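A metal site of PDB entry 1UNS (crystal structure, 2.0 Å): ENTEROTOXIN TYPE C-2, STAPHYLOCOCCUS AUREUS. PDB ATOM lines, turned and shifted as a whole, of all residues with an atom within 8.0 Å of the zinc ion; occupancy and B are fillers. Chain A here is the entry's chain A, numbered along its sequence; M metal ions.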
ATOM      1  N   ALA A  35      36.730   3.091  -3.390  1.00  0.00           N
ATOM      2  CA  ALA A  35      37.025   1.687  -3.639  1.00  0.00           C
ATOM      3  C   ALA A  35      35.951   1.124  -4.562  1.00  0.00           C
ATOM      4  O   ALA A  35      34.807   1.560  -4.545  1.00  0.00           O
ATOM      5  CB  ALA A  35      37.041   0.912  -2.328  1.00  0.00           C
ATOM      6  N   THR A  36      36.341   0.147  -5.370  1.00  0.00           N
ATOM      7  CA  THR A  36      35.412  -0.472  -6.306  1.00  0.00           C
ATOM      8  C   THR A  36      35.312  -1.970  -6.102  1.00  0.00           C
ATOM      9  O   THR A  36      36.325  -2.657  -5.927  1.00  0.00           O
ATOM     10  CB  THR A  36      35.834  -0.214  -7.769  1.00  0.00           C
ATOM     11  OG1 THR A  36      35.886   1.204  -8.009  1.00  0.00           O
ATOM     12  CG2 THR A  36      34.830  -0.835  -8.730  1.00  0.00           C
ATOM     13  N   LYS A  37      34.085  -2.474  -6.104  1.00  0.00           N
ATOM     14  CA  LYS A  37      33.803  -3.899  -5.975  1.00  0.00           C
ATOM     15  C   LYS A  37      34.530  -4.587  -4.815  1.00  0.00           C
ATOM     16  O   LYS A  37      35.251  -5.572  -5.029  1.00  0.00           O
ATOM     17  CB  LYS A  37      34.128  -4.598  -7.291  1.00  0.00           C
ATOM     18  CG  LYS A  37      33.218  -4.173  -8.434  1.00  0.00           C
ATOM     19  CD  LYS A  37      33.692  -4.687  -9.783  1.00  0.00           C
ATOM     20  CE  LYS A  37      33.654  -6.205  -9.836  1.00  0.00           C
ATOM     21  NZ  LYS A  37      34.208  -6.699 -11.127  1.00  0.00           N
ATOM     22  N   VAL A  38      34.320  -4.080  -3.606  1.00  0.00           N
ATOM     23  CA  VAL A  38      34.931  -4.647  -2.422  1.00  0.00           C
ATOM     24  C   VAL A  38      33.862  -5.270  -1.528  1.00  0.00           C
ATOM     25  O   VAL A  38      32.662  -5.024  -1.703  1.00  0.00           O
ATOM     26  CB  VAL A  38      35.716  -3.573  -1.616  1.00  0.00           C
ATOM     27  CG1 VAL A  38      36.924  -3.119  -2.421  1.00  0.00           C
ATOM     28  CG2 VAL A  38      34.810  -2.385  -1.302  1.00  0.00           C
ATOM     29  N   VAL A  81      28.913  -7.164  -2.784  1.00  0.00           N
ATOM     30  CA  VAL A  81      30.032  -6.532  -3.453  1.00  0.00           C
ATOM     31  C   VAL A  81      29.594  -5.074  -3.612  1.00  0.00           C
ATOM     32  O   VAL A  81      28.603  -4.789  -4.274  1.00  0.00           O
ATOM     33  CB  VAL A  81      30.278  -7.165  -4.839  1.00  0.00           C
ATOM     34  CG1 VAL A  81      31.392  -6.416  -5.588  1.00  0.00           C
ATOM     35  CG2 VAL A  81      30.659  -8.627  -4.676  1.00  0.00           C
ATOM     36  N   VAL A  82      30.331  -4.165  -2.988  1.00  0.00           N
ATOM     37  CA  VAL A  82      29.975  -2.749  -3.024  1.00  0.00           C
ATOM     38  C   VAL A  82      31.073  -1.788  -3.474  1.00  0.00           C
ATOM     39  O   VAL A  82      32.246  -2.147  -3.603  1.00  0.00           O
ATOM     40  CB  VAL A  82      29.506  -2.270  -1.634  1.00  0.00           C
ATOM     41  CG1 VAL A  82      28.371  -3.131  -1.140  1.00  0.00           C
ATOM     42  CG2 VAL A  82      30.678  -2.325  -0.656  1.00  0.00           C
ATOM     43  N   ASP A  83      30.648  -0.545  -3.711  1.00  0.00           N
ATOM     44  CA  ASP A  83      31.542   0.533  -4.090  1.00  0.00           C
ATOM     45  C   ASP A  83      31.556   1.463  -2.886  1.00  0.00           C
ATOM     46  O   ASP A  83      30.553   1.597  -2.196  1.00  0.00           O
ATOM     47  CB  ASP A  83      31.010   1.281  -5.309  1.00  0.00           C
ATOM     48  CG  ASP A  83      31.094   0.463  -6.576  1.00  0.00           C
ATOM     49  OD1 ASP A  83      30.333   0.764  -7.515  1.00  0.00           O
ATOM     50  OD2 ASP A  83      31.937  -0.456  -6.647  1.00  0.00           O
ATOM     51  N   VAL A  84      32.685   2.110  -2.635  1.00  0.00           N
ATOM     52  CA  VAL A  84      32.802   3.002  -1.487  1.00  0.00           C
ATOM     53  C   VAL A  84      33.314   4.375  -1.870  1.00  0.00           C
ATOM     54  O   VAL A  84      34.234   4.500  -2.679  1.00  0.00           O
ATOM     55  CB  VAL A  84      33.772   2.419  -0.425  1.00  0.00           C
ATOM     56  CG1 VAL A  84      33.851   3.342   0.777  1.00  0.00           C
ATOM     57  CG2 VAL A  84      33.315   1.043  -0.008  1.00  0.00           C
ATOM     58  N   THR A 116      27.471   1.866  -1.633  1.00  0.00           N
ATOM     59  CA  THR A 116      26.456   1.611  -2.645  1.00  0.00           C
ATOM     60  C   THR A 116      26.763   0.279  -3.327  1.00  0.00           C
ATOM     61  O   THR A 116      27.925  -0.065  -3.558  1.00  0.00           O
ATOM     62  CB  THR A 116      26.394   2.716  -3.737  1.00  0.00           C
ATOM     63  OG1 THR A 116      27.690   2.929  -4.296  1.00  0.00           O
ATOM     64  CG2 THR A 116      25.853   4.015  -3.140  1.00  0.00           C
ATOM     65  N   LYS A 117      25.712  -0.474  -3.624  1.00  0.00           N
ATOM     66  CA  LYS A 117      25.833  -1.760  -4.290  1.00  0.00           C
ATOM     67  C   LYS A 117      26.500  -1.484  -5.645  1.00  0.00           C
ATOM     68  O   LYS A 117      26.185  -0.488  -6.295  1.00  0.00           O
ATOM     69  CB  LYS A 117      24.429  -2.331  -4.482  1.00  0.00           C
ATOM     70  CG  LYS A 117      24.329  -3.760  -4.982  1.00  0.00           C
ATOM     71  CD  LYS A 117      22.856  -4.185  -5.056  1.00  0.00           C
ATOM     72  CE  LYS A 117      22.684  -5.624  -5.509  1.00  0.00           C
ATOM     73  NZ  LYS A 117      21.245  -5.990  -5.657  1.00  0.00           N
ATOM     74  N   HIS A 118      27.419  -2.337  -6.072  1.00  0.00           N
ATOM     75  CA  HIS A 118      28.060  -2.133  -7.366  1.00  0.00           C
ATOM     76  C   HIS A 118      27.161  -2.608  -8.517  1.00  0.00           C
ATOM     77  O   HIS A 118      27.017  -1.924  -9.538  1.00  0.00           O
ATOM     78  CB  HIS A 118      29.396  -2.881  -7.426  1.00  0.00           C
ATOM     79  CG  HIS A 118      29.919  -3.080  -8.815  1.00  0.00           C
ATOM     80  ND1 HIS A 118      30.508  -2.070  -9.535  1.00  0.00           N
ATOM     81  CD2 HIS A 118      29.895  -4.164  -9.625  1.00  0.00           C
ATOM     82  CE1 HIS A 118      30.838  -2.520 -10.737  1.00  0.00           C
ATOM     83  NE2 HIS A 118      30.481  -3.788 -10.820  1.00  0.00           N
ATOM     84  N   GLU A 119      26.552  -3.786  -8.322  1.00  0.00           N
ATOM     85  CA  GLU A 119      25.665  -4.374  -9.329  1.00  0.00           C
ATOM     86  C   GLU A 119      24.475  -3.523  -9.719  1.00  0.00           C
ATOM     87  O   GLU A 119      23.731  -3.069  -8.843  1.00  0.00           O
ATOM     88  CB  GLU A 119      25.135  -5.715  -8.836  1.00  0.00           C
ATOM     89  CG  GLU A 119      26.171  -6.771  -8.631  1.00  0.00           C
ATOM     90  CD  GLU A 119      25.592  -7.954  -7.894  1.00  0.00           C
ATOM     91  OE1 GLU A 119      25.169  -7.770  -6.728  1.00  0.00           O
ATOM     92  OE2 GLU A 119      25.551  -9.058  -8.485  1.00  0.00           O
ATOM     93  N   GLY A 120      24.290  -3.339 -11.017  1.00  0.00           N
ATOM     94  CA  GLY A 120      23.170  -2.566 -11.535  1.00  0.00           C
ATOM     95  C   GLY A 120      23.120  -1.110 -11.104  1.00  0.00           C
ATOM     96  O   GLY A 120      22.069  -0.475 -11.198  1.00  0.00           O
ATOM     97  N   ASN A 121      24.245  -0.556 -10.646  1.00  0.00           N
ATOM     98  CA  ASN A 121      24.238   0.835 -10.215  1.00  0.00           C
ATOM     99  C   ASN A 121      25.018   1.792 -11.130  1.00  0.00           C
ATOM    100  O   ASN A 121      25.308   2.934 -10.747  1.00  0.00           O
ATOM    101  CB  ASN A 121      24.799   0.952  -8.784  1.00  0.00           C
ATOM    102  CG  ASN A 121      24.433   2.258  -8.124  1.00  0.00           C
ATOM    103  OD1 ASN A 121      25.211   2.814  -7.352  1.00  0.00           O
ATOM    104  ND2 ASN A 121      23.248   2.760  -8.422  1.00  0.00           N
ATOM    105  N   HIS A 122      25.344   1.330 -12.336  1.00  0.00           N
ATOM    106  CA  HIS A 122      26.079   2.163 -13.303  1.00  0.00           C
ATOM    107  C   HIS A 122      25.320   2.328 -14.615  1.00  0.00           C
ATOM    108  O   HIS A 122      24.477   1.506 -14.968  1.00  0.00           O
ATOM    109  CB  HIS A 122      27.471   1.560 -13.564  1.00  0.00           C
ATOM    110  CG  HIS A 122      28.322   1.458 -12.329  1.00  0.00           C
ATOM    111  ND1 HIS A 122      28.727   2.571 -11.612  1.00  0.00           N
ATOM    112  CD2 HIS A 122      28.800   0.387 -11.662  1.00  0.00           C
ATOM    113  CE1 HIS A 122      29.422   2.176 -10.564  1.00  0.00           C
ATOM    114  NE2 HIS A 122      29.480   0.851 -10.564  1.00  0.00           N
ATOM    115  N   ASP A 150      29.468   8.253 -11.582  1.00  0.00           N
ATOM    116  CA  ASP A 150      29.194   7.128 -12.461  1.00  0.00           C
ATOM    117  C   ASP A 150      28.108   6.233 -11.870  1.00  0.00           C
ATOM    118  O   ASP A 150      27.772   5.196 -12.423  1.00  0.00           O
ATOM    119  CB  ASP A 150      30.471   6.314 -12.659  1.00  0.00           C
ATOM    120  CG  ASP A 150      31.014   5.747 -11.358  1.00  0.00           C
ATOM    121  OD1 ASP A 150      31.845   4.830 -11.421  1.00  0.00           O
ATOM    122  OD2 ASP A 150      30.622   6.228 -10.272  1.00  0.00           O
ATOM    123  N   LYS A 151      27.550   6.648 -10.732  1.00  0.00           N
ATOM    124  CA  LYS A 151      26.517   5.870 -10.061  1.00  0.00           C
ATOM    125  C   LYS A 151      25.087   6.391 -10.286  1.00  0.00           C
ATOM    126  O   LYS A 151      24.870   7.602 -10.321  1.00  0.00           O
ATOM    127  CB  LYS A 151      26.789   5.855  -8.548  1.00  0.00           C
ATOM    128  CG  LYS A 151      28.186   5.396  -8.173  1.00  0.00           C
ATOM    129  CD  LYS A 151      28.401   5.465  -6.655  1.00  0.00           C
ATOM    130  CE  LYS A 151      29.794   4.979  -6.268  1.00  0.00           C
ATOM    131  NZ  LYS A 151      30.866   5.937  -6.653  1.00  0.00           N
HETATM  132 ZN    ZN M   1      30.713  -0.010  -9.223  1.00  0.00          ZN
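The backbone carbonyl oxygen of Thr 116 is in hydrogen-bond range of the backbone NH of Asp 83 (2.8 Å). OD2 of Asp 83 is in hydrogen-bond range of N of Lys 37 (3.0 Å). A ring nitrogen (ND1) of His 122 lies within hydrogen-bond range of the backbone carbonyl oxygen of Asp 150 (2.9 Å). N of His 118 is in hydrogen-bond range of O of Val 81, 3.3 Å away.
Three residues have an atom within 4 Å of the zinc ion: Asp 83, His 118 and His 122. The nearest printed residue that does not touch the zinc ion is Thr 36 (4.2 Å).
The zinc ion is bound by OD1 of Asp 83 (1.9 Å), NE2 of His 122 (2.0 Å) and ND1 of His 118 (2.1 Å).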
